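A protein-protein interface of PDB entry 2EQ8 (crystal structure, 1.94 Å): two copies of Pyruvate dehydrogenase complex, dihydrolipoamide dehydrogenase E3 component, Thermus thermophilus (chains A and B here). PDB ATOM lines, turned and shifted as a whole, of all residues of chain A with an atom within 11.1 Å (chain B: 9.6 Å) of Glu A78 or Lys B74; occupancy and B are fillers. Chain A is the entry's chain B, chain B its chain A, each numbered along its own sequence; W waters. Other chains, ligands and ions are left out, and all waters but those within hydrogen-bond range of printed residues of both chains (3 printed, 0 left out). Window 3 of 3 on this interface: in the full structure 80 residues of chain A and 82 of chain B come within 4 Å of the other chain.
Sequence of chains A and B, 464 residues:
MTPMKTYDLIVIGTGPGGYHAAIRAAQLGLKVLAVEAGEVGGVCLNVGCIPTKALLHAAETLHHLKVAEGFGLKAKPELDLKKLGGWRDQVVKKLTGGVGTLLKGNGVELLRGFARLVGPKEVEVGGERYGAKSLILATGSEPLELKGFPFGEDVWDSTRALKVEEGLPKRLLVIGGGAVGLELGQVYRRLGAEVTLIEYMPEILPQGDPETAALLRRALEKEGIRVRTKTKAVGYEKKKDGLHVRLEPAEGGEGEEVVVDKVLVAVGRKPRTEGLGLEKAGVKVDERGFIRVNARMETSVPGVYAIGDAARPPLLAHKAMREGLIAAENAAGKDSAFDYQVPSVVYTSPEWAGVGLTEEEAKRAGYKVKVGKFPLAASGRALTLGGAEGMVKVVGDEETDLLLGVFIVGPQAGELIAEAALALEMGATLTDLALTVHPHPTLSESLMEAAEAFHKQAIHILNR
Of the 22 printed residues of chain A, 11 touch a printed residue of chain B.
Hydrophobic or aromatic side chains of chain A that line the printed part of chain B: Ala A58, Leu A62, Leu A79 and Leu A84.
Printed residues of chain B that touch a printed residue of chain A: Gly B70, Phe B71, Gly B72, Leu B73, Lys B74, Lys B76 and Pro B77.
Hydrophobic or aromatic side chains of chain B that line the printed part of chain A: Phe B71 and Leu B73.
Among the printed residues, Asp or Glu carboxylates within 4 Å of a Lys or Arg side-chain nitrogen of the other chain: Glu A78 with Lys B74.
Lys A74 touches Lys B76, and with the chains exchanged Lys A76 touches Lys B74.
Lys A74 touches Pro B77, and with the chains exchanged Pro A77 touches Lys B74.
Of the 19 pairs that touch across the chains among the printed residues, 4 have their exchanged pair printed and touching as well.
Among the printed residues, merely in contact across the chains: Ala A58 with Phe B71 (3.7 Å), Thr A61 with Phe B71 (3.9 Å), Thr A61 with Leu B73 (3.6 Å), Leu A62 with Leu B73 (3.5 Å), Lys A74 with Lys B76 (3.9 Å), Lys A74 with Pro B77 (3.4 Å), Lys A76 with Lys B74 (3.8 Å), Pro A77 with Lys B74 (3.6 Å), Glu A78 with Leu B73 (3.8 Å), Leu A79 with Phe B71 (3.7 Å), Leu A79 with Gly B72 (3.2 Å), Leu A79 with Leu B73 (3.6 Å), Lys A83 with Gly B70 (3.9 Å), Lys A83 with Phe B71 (3.9 Å), Lys A83 with Gly B72 (3.3 Å) and Leu A84 with Phe B71 (3.2 Å).
O of Gly B72 sits at hydrogen-bond distance from N of Asp A80 (2.7 Å).
The side-chain amino group of Lys B74 is in salt-bridge range of the side-chain carboxylate of Glu A78, at 2.8 Å.
O of Glu A78 sits close to O of Gly B72, 3.1 Å away.
Water W1 lies within hydrogen-bond range of N of Lys B76 and N of Lys A76.
Water W2 bridges O of Glu A78 and NZ of Lys B74.
Water W3 lies within hydrogen-bond range of O of Lys B74 (2.9 Å) and O of Lys A76 (3.1 Å).
Printed residues of chain B within 4 Å of Thr A61: Phe B71 (3.9 Å) and Leu B73 (3.6 Å).
Leu A65 touches none of the printed residues of chain B.
Lys A66 touches none of the printed residues of chain B.
Glu A78 touches three residues of chain B.
Of the printed residues of chain B, Leu A84 touches Phe B71.
No residue of chain A comes within 4 Å of Glu B69.
Gly B72 touches four residues of chain A.
No residue of chain A comes within 4 Å of Ala B75.
Of the printed residues of chain A, Pro B77 touches Lys A74 (3.4 Å).
The nearest residue of chain A that does not touch Lys B74 is Leu A79 (4.9 Å).
The backbone carbonyl oxygen (O) of Ala B68 is in hydrogen-bond range of the backbone NH (N) of Leu B73.
The side-chain carboxylate (OD1) of Asp A80 sits at hydrogen-bond distance from the backbone NH (N) of Lys A82 (3.0 Å).
OD1 of Asp A80 sits at hydrogen-bond distance from N of Lys A83 (3.2 Å).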
ATOM      1  N   ALA A  58      15.045 -26.782   3.537  1.00  0.00           N
ATOM      2  CA  ALA A  58      15.314 -25.715   4.500  1.00  0.00           C
ATOM      3  C   ALA A  58      15.688 -24.435   3.748  1.00  0.00           C
ATOM      4  O   ALA A  58      15.260 -23.339   4.111  1.00  0.00           O
ATOM      5  CB  ALA A  58      16.451 -26.118   5.438  1.00  0.00           C
ATOM      6  N   ALA A  59      16.481 -24.587   2.696  1.00  0.00           N
ATOM      7  CA  ALA A  59      16.924 -23.447   1.894  1.00  0.00           C
ATOM      8  C   ALA A  59      15.757 -22.770   1.191  1.00  0.00           C
ATOM      9  O   ALA A  59      15.676 -21.540   1.144  1.00  0.00           O
ATOM     10  CB  ALA A  59      17.958 -23.907   0.873  1.00  0.00           C
ATOM     11  N   THR A  61      12.665 -22.893   2.132  1.00  0.00           N
ATOM     12  CA  THR A  61      11.813 -22.281   3.139  1.00  0.00           C
ATOM     13  C   THR A  61      12.345 -20.885   3.468  1.00  0.00           C
ATOM     14  O   THR A  61      11.580 -19.923   3.546  1.00  0.00           O
ATOM     15  CB  THR A  61      11.758 -23.137   4.428  1.00  0.00           C
ATOM     16  OG1 THR A  61      11.266 -24.446   4.109  1.00  0.00           O
ATOM     17  CG2 THR A  61      10.822 -22.501   5.450  1.00  0.00           C
ATOM     18  N   LEU A  62      13.656 -20.776   3.653  1.00  0.00           N
ATOM     19  CA  LEU A  62      14.278 -19.487   3.955  1.00  0.00           C
ATOM     20  C   LEU A  62      14.124 -18.545   2.760  1.00  0.00           C
ATOM     21  O   LEU A  62      13.671 -17.409   2.895  1.00  0.00           O
ATOM     22  CB  LEU A  62      15.762 -19.692   4.268  1.00  0.00           C
ATOM     23  CG  LEU A  62      16.621 -18.435   4.442  1.00  0.00           C
ATOM     24  CD1 LEU A  62      16.156 -17.627   5.654  1.00  0.00           C
ATOM     25  CD2 LEU A  62      18.072 -18.856   4.601  1.00  0.00           C
ATOM     26  N   HIS A  63      14.503 -19.036   1.585  1.00  0.00           N
ATOM     27  CA  HIS A  63      14.415 -18.261   0.351  1.00  0.00           C
ATOM     28  C   HIS A  63      13.024 -17.691   0.076  1.00  0.00           C
ATOM     29  O   HIS A  63      12.879 -16.518  -0.268  1.00  0.00           O
ATOM     30  CB  HIS A  63      14.822 -19.134  -0.839  1.00  0.00           C
ATOM     31  CG  HIS A  63      14.714 -18.440  -2.160  1.00  0.00           C
ATOM     32  ND1 HIS A  63      15.624 -17.494  -2.581  1.00  0.00           N
ATOM     33  CD2 HIS A  63      13.797 -18.543  -3.150  1.00  0.00           C
ATOM     34  CE1 HIS A  63      15.274 -17.045  -3.771  1.00  0.00           C
ATOM     35  NE2 HIS A  63      14.168 -17.666  -4.140  1.00  0.00           N
ATOM     36  N   LEU A  65      10.785 -16.701   1.929  1.00  0.00           N
ATOM     37  CA  LEU A  65      10.383 -15.600   2.798  1.00  0.00           C
ATOM     38  C   LEU A  65      10.543 -14.237   2.131  1.00  0.00           C
ATOM     39  O   LEU A  65       9.874 -13.277   2.502  1.00  0.00           O
ATOM     40  CB  LEU A  65      11.177 -15.643   4.106  1.00  0.00           C
ATOM     41  CG  LEU A  65      10.837 -16.849   4.987  1.00  0.00           C
ATOM     42  CD1 LEU A  65      11.682 -16.843   6.252  1.00  0.00           C
ATOM     43  CD2 LEU A  65       9.357 -16.800   5.330  1.00  0.00           C
ATOM     44  N   LYS A  66      11.430 -14.151   1.147  1.00  0.00           N
ATOM     45  CA  LYS A  66      11.635 -12.891   0.441  1.00  0.00           C
ATOM     46  C   LYS A  66      10.382 -12.574  -0.374  1.00  0.00           C
ATOM     47  O   LYS A  66       9.905 -11.436  -0.387  1.00  0.00           O
ATOM     48  CB  LYS A  66      12.876 -12.987  -0.451  1.00  0.00           C
ATOM     49  CG  LYS A  66      14.136 -13.308   0.343  1.00  0.00           C
ATOM     50  CD  LYS A  66      15.413 -13.148  -0.465  1.00  0.00           C
ATOM     51  CE  LYS A  66      15.505 -14.153  -1.596  1.00  0.00           C
ATOM     52  NZ  LYS A  66      16.805 -14.016  -2.311  1.00  0.00           N
ATOM     53  N   GLU A  69       7.365 -11.579   1.877  1.00  0.00           N
ATOM     54  CA  GLU A  69       7.251 -10.211   2.377  1.00  0.00           C
ATOM     55  C   GLU A  69       6.238  -9.501   1.484  1.00  0.00           C
ATOM     56  O   GLU A  69       5.522  -8.602   1.924  1.00  0.00           O
ATOM     57  CB  GLU A  69       8.602  -9.485   2.312  1.00  0.00           C
ATOM     58  CG  GLU A  69       9.670 -10.076   3.212  1.00  0.00           C
ATOM     59  CD  GLU A  69      10.858  -9.143   3.396  1.00  0.00           C
ATOM     60  OE1 GLU A  69      11.406  -8.656   2.386  1.00  0.00           O
ATOM     61  OE2 GLU A  69      11.245  -8.902   4.557  1.00  0.00           O
ATOM     62  N   LYS A  74       6.165 -10.478   7.434  1.00  0.00           N
ATOM     63  CA  LYS A  74       7.348  -9.756   7.876  1.00  0.00           C
ATOM     64  C   LYS A  74       8.149 -10.640   8.816  1.00  0.00           C
ATOM     65  O   LYS A  74       7.598 -11.242   9.735  1.00  0.00           O
ATOM     66  CB  LYS A  74       6.942  -8.466   8.585  1.00  0.00           C
ATOM     67  N   ALA A  75       9.451 -10.719   8.583  1.00  0.00           N
ATOM     68  CA  ALA A  75      10.303 -11.543   9.421  1.00  0.00           C
ATOM     69  C   ALA A  75      11.776 -11.229   9.205  1.00  0.00           C
ATOM     70  O   ALA A  75      12.180 -10.760   8.141  1.00  0.00           O
ATOM     71  CB  ALA A  75      10.041 -13.022   9.131  1.00  0.00           C
ATOM     72  N   LYS A  76      12.569 -11.486  10.237  1.00  0.00           N
ATOM     73  CA  LYS A  76      14.006 -11.285  10.176  1.00  0.00           C
ATOM     74  C   LYS A  76      14.599 -12.663  10.445  1.00  0.00           C
ATOM     75  O   LYS A  76      15.021 -12.969  11.559  1.00  0.00           O
ATOM     76  CB  LYS A  76      14.456 -10.273  11.235  1.00  0.00           C
ATOM     77  CG  LYS A  76      13.866  -8.885  11.023  1.00  0.00           C
ATOM     78  CD  LYS A  76      14.516  -7.846  11.922  1.00  0.00           C
ATOM     79  CE  LYS A  76      13.939  -6.460  11.660  1.00  0.00           C
ATOM     80  NZ  LYS A  76      12.488  -6.394  12.001  1.00  0.00           N
ATOM     81  N   PRO A  77      14.624 -13.519   9.411  1.00  0.00           N
ATOM     82  CA  PRO A  77      15.149 -14.883   9.500  1.00  0.00           C
ATOM     83  C   PRO A  77      16.624 -15.014   9.856  1.00  0.00           C
ATOM     84  O   PRO A  77      17.474 -14.268   9.370  1.00  0.00           O
ATOM     85  CB  PRO A  77      14.832 -15.461   8.125  1.00  0.00           C
ATOM     86  CG  PRO A  77      14.966 -14.277   7.236  1.00  0.00           C
ATOM     87  CD  PRO A  77      14.241 -13.200   8.023  1.00  0.00           C
ATOM     88  N   GLU A  78      16.906 -15.980  10.723  1.00  0.00           N
ATOM     89  CA  GLU A  78      18.260 -16.276  11.169  1.00  0.00           C
ATOM     90  C   GLU A  78      18.355 -17.801  11.182  1.00  0.00           C
ATOM     91  O   GLU A  78      17.688 -18.461  11.976  1.00  0.00           O
ATOM     92  CB  GLU A  78      18.485 -15.707  12.574  1.00  0.00           C
ATOM     93  CG  GLU A  78      19.776 -16.141  13.239  1.00  0.00           C
ATOM     94  CD  GLU A  78      19.957 -15.516  14.612  1.00  0.00           C
ATOM     95  OE1 GLU A  78      20.837 -15.978  15.369  1.00  0.00           O
ATOM     96  OE2 GLU A  78      19.219 -14.557  14.928  1.00  0.00           O
ATOM     97  N   LEU A  79      19.170 -18.354  10.289  1.00  0.00           N
ATOM     98  CA  LEU A  79      19.316 -19.802  10.187  1.00  0.00           C
ATOM     99  C   LEU A  79      20.519 -20.360  10.935  1.00  0.00           C
ATOM    100  O   LEU A  79      21.666 -20.055  10.616  1.00  0.00           O
ATOM    101  CB  LEU A  79      19.387 -20.215   8.713  1.00  0.00           C
ATOM    102  CG  LEU A  79      19.417 -21.716   8.407  1.00  0.00           C
ATOM    103  CD1 LEU A  79      18.189 -22.387   8.992  1.00  0.00           C
ATOM    104  CD2 LEU A  79      19.472 -21.928   6.906  1.00  0.00           C
ATOM    105  N   ASP A  80      20.237 -21.185  11.938  1.00  0.00           N
ATOM    106  CA  ASP A  80      21.269 -21.824  12.747  1.00  0.00           C
ATOM    107  C   ASP A  80      21.738 -23.067  11.992  1.00  0.00           C
ATOM    108  O   ASP A  80      21.021 -24.069  11.941  1.00  0.00           O
ATOM    109  CB  ASP A  80      20.672 -22.229  14.098  1.00  0.00           C
ATOM    110  CG  ASP A  80      21.698 -22.817  15.040  1.00  0.00           C
ATOM    111  OD1 ASP A  80      22.707 -23.371  14.561  1.00  0.00           O
ATOM    112  OD2 ASP A  80      21.484 -22.734  16.266  1.00  0.00           O
ATOM    113  N   LEU A  81      22.935 -23.008  11.413  1.00  0.00           N
ATOM    114  CA  LEU A  81      23.470 -24.131  10.638  1.00  0.00           C
ATOM    115  C   LEU A  81      23.714 -25.412  11.438  1.00  0.00           C
ATOM    116  O   LEU A  81      23.609 -26.518  10.901  1.00  0.00           O
ATOM    117  CB  LEU A  81      24.761 -23.714   9.931  1.00  0.00           C
ATOM    118  CG  LEU A  81      24.612 -22.534   8.966  1.00  0.00           C
ATOM    119  CD1 LEU A  81      25.977 -22.150   8.422  1.00  0.00           C
ATOM    120  CD2 LEU A  81      23.656 -22.896   7.830  1.00  0.00           C
ATOM    121  N   LYS A  82      24.054 -25.278  12.713  1.00  0.00           N
ATOM    122  CA  LYS A  82      24.279 -26.464  13.529  1.00  0.00           C
ATOM    123  C   LYS A  82      22.939 -27.160  13.755  1.00  0.00           C
ATOM    124  O   LYS A  82      22.845 -28.386  13.709  1.00  0.00           O
ATOM    125  CB  LYS A  82      24.918 -26.087  14.870  1.00  0.00           C
ATOM    126  CG  LYS A  82      26.309 -25.477  14.736  1.00  0.00           C
ATOM    127  CD  LYS A  82      26.957 -25.198  16.093  1.00  0.00           C
ATOM    128  CE  LYS A  82      27.336 -26.482  16.831  1.00  0.00           C
ATOM    129  NZ  LYS A  82      26.155 -27.294  17.250  1.00  0.00           N
ATOM    130  N   LYS A  83      21.901 -26.368  13.996  1.00  0.00           N
ATOM    131  CA  LYS A  83      20.567 -26.909  14.216  1.00  0.00           C
ATOM    132  C   LYS A  83      20.063 -27.563  12.927  1.00  0.00           C
ATOM    133  O   LYS A  83      19.398 -28.604  12.963  1.00  0.00           O
ATOM    134  CB  LYS A  83      19.615 -25.792  14.629  1.00  0.00           C
ATOM    135  CG  LYS A  83      18.223 -26.261  15.024  1.00  0.00           C
ATOM    136  CD  LYS A  83      17.983 -26.062  16.510  1.00  0.00           C
ATOM    137  CE  LYS A  83      18.157 -24.601  16.900  1.00  0.00           C
ATOM    138  NZ  LYS A  83      17.983 -24.382  18.364  1.00  0.00           N
ATOM    139  N   LEU A  84      20.379 -26.944  11.791  1.00  0.00           N
ATOM    140  CA  LEU A  84      19.966 -27.482  10.496  1.00  0.00           C
ATOM    141  C   LEU A  84      20.620 -28.836  10.267  1.00  0.00           C
ATOM    142  O   LEU A  84      19.961 -29.798   9.866  1.00  0.00           O
ATOM    143  CB  LEU A  84      20.354 -26.520   9.369  1.00  0.00           C
ATOM    144  CG  LEU A  84      20.164 -27.034   7.938  1.00  0.00           C
ATOM    145  CD1 LEU A  84      18.740 -27.576   7.765  1.00  0.00           C
ATOM    146  CD2 LEU A  84      20.446 -25.906   6.944  1.00  0.00           C
ATOM    147  N   ARG A 190      21.951 -20.284  -1.432  1.00  0.00           N
ATOM    148  CA  ARG A 190      20.881 -19.825  -0.557  1.00  0.00           C
ATOM    149  C   ARG A 190      21.312 -19.673   0.896  1.00  0.00           C
ATOM    150  O   ARG A 190      20.703 -18.914   1.656  1.00  0.00           O
ATOM    151  CB  ARG A 190      19.676 -20.764  -0.678  1.00  0.00           C
ATOM    152  CG  ARG A 190      19.100 -20.737  -2.087  1.00  0.00           C
ATOM    153  CD  ARG A 190      17.835 -21.547  -2.263  1.00  0.00           C
ATOM    154  NE  ARG A 190      17.111 -21.045  -3.427  1.00  0.00           N
ATOM    155  CZ  ARG A 190      15.867 -21.370  -3.745  1.00  0.00           C
ATOM    156  NH1 ARG A 190      15.183 -22.221  -2.991  1.00  0.00           N
ATOM    157  NH2 ARG A 190      15.291 -20.802  -4.798  1.00  0.00           N
ATOM    158  N   LEU A 191      22.369 -20.383   1.279  1.00  0.00           N
ATOM    159  CA  LEU A 191      22.865 -20.298   2.647  1.00  0.00           C
ATOM    160  C   LEU A 191      23.838 -19.134   2.831  1.00  0.00           C
ATOM    161  O   LEU A 191      24.370 -18.931   3.920  1.00  0.00           O
ATOM    162  CB  LEU A 191      23.519 -21.618   3.068  1.00  0.00           C
ATOM    163  CG  LEU A 191      22.543 -22.791   3.231  1.00  0.00           C
ATOM    164  CD1 LEU A 191      23.265 -23.985   3.820  1.00  0.00           C
ATOM    165  CD2 LEU A 191      21.387 -22.379   4.132  1.00  0.00           C
ATOM    166  N   GLY A 192      24.072 -18.374   1.764  1.00  0.00           N
ATOM    167  CA  GLY A 192      24.938 -17.213   1.875  1.00  0.00           C
ATOM    168  C   GLY A 192      26.265 -17.175   1.140  1.00  0.00           C
ATOM    169  O   GLY A 192      26.980 -16.178   1.230  1.00  0.00           O
ATOM    170  N   LEU B  65       6.557 -22.232   9.350  1.00  0.00           N
ATOM    171  CA  LEU B  65       7.721 -21.666  10.038  1.00  0.00           C
ATOM    172  C   LEU B  65       7.890 -22.265  11.433  1.00  0.00           C
ATOM    173  O   LEU B  65       8.977 -22.226  12.010  1.00  0.00           O
ATOM    174  CB  LEU B  65       7.602 -20.138  10.117  1.00  0.00           C
ATOM    175  CG  LEU B  65       7.693 -19.449   8.747  1.00  0.00           C
ATOM    176  CD1 LEU B  65       7.533 -17.943   8.891  1.00  0.00           C
ATOM    177  CD2 LEU B  65       9.040 -19.769   8.115  1.00  0.00           C
ATOM    178  N   LYS B  66       6.812 -22.826  11.969  1.00  0.00           N
ATOM    179  CA  LYS B  66       6.852 -23.455  13.284  1.00  0.00           C
ATOM    180  C   LYS B  66       7.704 -24.721  13.174  1.00  0.00           C
ATOM    181  O   LYS B  66       8.562 -24.987  14.021  1.00  0.00           O
ATOM    182  CB  LYS B  66       5.429 -23.789  13.741  1.00  0.00           C
ATOM    183  CG  LYS B  66       4.557 -22.553  13.922  1.00  0.00           C
ATOM    184  CD  LYS B  66       3.113 -22.903  14.243  1.00  0.00           C
ATOM    185  CE  LYS B  66       2.270 -21.642  14.391  1.00  0.00           C
ATOM    186  NZ  LYS B  66       0.845 -21.964  14.700  1.00  0.00           N
ATOM    187  N   VAL B  67       7.471 -25.494  12.117  1.00  0.00           N
ATOM    188  CA  VAL B  67       8.241 -26.707  11.885  1.00  0.00           C
ATOM    189  C   VAL B  67       9.669 -26.322  11.522  1.00  0.00           C
ATOM    190  O   VAL B  67      10.624 -27.000  11.909  1.00  0.00           O
ATOM    191  CB  VAL B  67       7.627 -27.555  10.737  1.00  0.00           C
ATOM    192  CG1 VAL B  67       8.674 -28.480  10.140  1.00  0.00           C
ATOM    193  CG2 VAL B  67       6.468 -28.375  11.276  1.00  0.00           C
ATOM    194  N   ALA B  68       9.806 -25.220  10.790  1.00  0.00           N
ATOM    195  CA  ALA B  68      11.111 -24.722  10.357  1.00  0.00           C
ATOM    196  C   ALA B  68      12.025 -24.358  11.528  1.00  0.00           C
ATOM    197  O   ALA B  68      13.250 -24.447  11.416  1.00  0.00           O
ATOM    198  CB  ALA B  68      10.930 -23.512   9.443  1.00  0.00           C
ATOM    199  N   GLU B  69      11.440 -23.935  12.642  1.00  0.00           N
ATOM    200  CA  GLU B  69      12.250 -23.599  13.807  1.00  0.00           C
ATOM    201  C   GLU B  69      13.018 -24.867  14.180  1.00  0.00           C
ATOM    202  O   GLU B  69      14.139 -24.814  14.687  1.00  0.00           O
ATOM    203  CB  GLU B  69      11.358 -23.169  14.973  1.00  0.00           C
ATOM    204  CG  GLU B  69      12.137 -22.536  16.105  1.00  0.00           C
ATOM    205  CD  GLU B  69      12.444 -21.066  15.861  1.00  0.00           C
ATOM    206  OE1 GLU B  69      13.526 -20.615  16.279  1.00  0.00           O
ATOM    207  OE2 GLU B  69      11.600 -20.358  15.268  1.00  0.00           O
ATOM    208  N   GLY B  70      12.391 -26.009  13.908  1.00  0.00           N
ATOM    209  CA  GLY B  70      12.992 -27.299  14.194  1.00  0.00           C
ATOM    210  C   GLY B  70      14.276 -27.558  13.433  1.00  0.00           C
ATOM    211  O   GLY B  70      15.103 -28.366  13.868  1.00  0.00           O
ATOM    212  N   PHE B  71      14.448 -26.918  12.279  1.00  0.00           N
ATOM    213  CA  PHE B  71      15.691 -27.110  11.551  1.00  0.00           C
ATOM    214  C   PHE B  71      16.561 -25.860  11.497  1.00  0.00           C
ATOM    215  O   PHE B  71      17.321 -25.643  10.551  1.00  0.00           O
ATOM    216  CB  PHE B  71      15.467 -27.721  10.148  1.00  0.00           C
ATOM    217  CG  PHE B  71      14.471 -27.004   9.280  1.00  0.00           C
ATOM    218  CD1 PHE B  71      14.743 -25.739   8.764  1.00  0.00           C
ATOM    219  CD2 PHE B  71      13.294 -27.647   8.889  1.00  0.00           C
ATOM    220  CE1 PHE B  71      13.861 -25.130   7.864  1.00  0.00           C
ATOM    221  CE2 PHE B  71      12.405 -27.044   7.990  1.00  0.00           C
ATOM    222  CZ  PHE B  71      12.690 -25.787   7.477  1.00  0.00           C
ATOM    223  N   GLY B  72      16.440 -25.046  12.543  1.00  0.00           N
ATOM    224  CA  GLY B  72      17.263 -23.856  12.675  1.00  0.00           C
ATOM    225  C   GLY B  72      16.804 -22.521  12.132  1.00  0.00           C
ATOM    226  O   GLY B  72      17.537 -21.541  12.242  1.00  0.00           O
ATOM    227  N   LEU B  73      15.616 -22.457  11.546  1.00  0.00           N
ATOM    228  CA  LEU B  73      15.140 -21.194  10.997  1.00  0.00           C
ATOM    229  C   LEU B  73      14.392 -20.447  12.093  1.00  0.00           C
ATOM    230  O   LEU B  73      13.235 -20.745  12.390  1.00  0.00           O
ATOM    231  CB  LEU B  73      14.231 -21.450   9.790  1.00  0.00           C
ATOM    232  CG  LEU B  73      13.881 -20.249   8.906  1.00  0.00           C
ATOM    233  CD1 LEU B  73      15.153 -19.610   8.375  1.00  0.00           C
ATOM    234  CD2 LEU B  73      13.006 -20.709   7.752  1.00  0.00           C
ATOM    235  N   LYS B  74      15.072 -19.484  12.706  1.00  0.00           N
ATOM    236  CA  LYS B  74      14.477 -18.704  13.779  1.00  0.00           C
ATOM    237  C   LYS B  74      14.024 -17.339  13.290  1.00  0.00           C
ATOM    238  O   LYS B  74      14.755 -16.632  12.593  1.00  0.00           O
ATOM    239  CB  LYS B  74      15.473 -18.548  14.935  1.00  0.00           C
ATOM    240  CG  LYS B  74      15.045 -17.560  16.017  1.00  0.00           C
ATOM    241  CD  LYS B  74      15.856 -17.732  17.305  1.00  0.00           C
ATOM    242  CE  LYS B  74      17.360 -17.718  17.048  1.00  0.00           C
ATOM    243  NZ  LYS B  74      17.827 -16.460  16.396  1.00  0.00           N
ATOM    244  N   ALA B  75      12.802 -16.981  13.661  1.00  0.00           N
ATOM    245  CA  ALA B  75      12.230 -15.704  13.278  1.00  0.00           C
ATOM    246  C   ALA B  75      10.956 -15.454  14.071  1.00  0.00           C
ATOM    247  O   ALA B  75      10.393 -16.365  14.684  1.00  0.00           O
ATOM    248  CB  ALA B  75      11.930 -15.694  11.777  1.00  0.00           C
ATOM    249  N   LYS B  76      10.522 -14.203  14.075  1.00  0.00           N
ATOM    250  CA  LYS B  76       9.304 -13.810  14.759  1.00  0.00           C
ATOM    251  C   LYS B  76       8.402 -13.325  13.636  1.00  0.00           C
ATOM    252  O   LYS B  76       8.232 -12.126  13.442  1.00  0.00           O
ATOM    253  CB  LYS B  76       9.589 -12.676  15.747  1.00  0.00           C
ATOM    254  N   PRO B  77       7.822 -14.265  12.870  1.00  0.00           N
ATOM    255  CA  PRO B  77       6.941 -13.908  11.757  1.00  0.00           C
ATOM    256  C   PRO B  77       5.685 -13.170  12.193  1.00  0.00           C
ATOM    257  O   PRO B  77       5.060 -13.521  13.191  1.00  0.00           O
ATOM    258  CB  PRO B  77       6.637 -15.260  11.116  1.00  0.00           C
ATOM    259  CG  PRO B  77       6.608 -16.176  12.300  1.00  0.00           C
ATOM    260  CD  PRO B  77       7.822 -15.723  13.090  1.00  0.00           C
HETATM  261  O   HOH W   1      11.691 -12.028  13.201  1.00  0.00           O
HETATM  262  O   HOH W   2      18.727 -18.613  14.513  1.00  0.00           O
HETATM  263  O   HOH W   3      15.501 -14.350  14.284  1.00  0.00           O
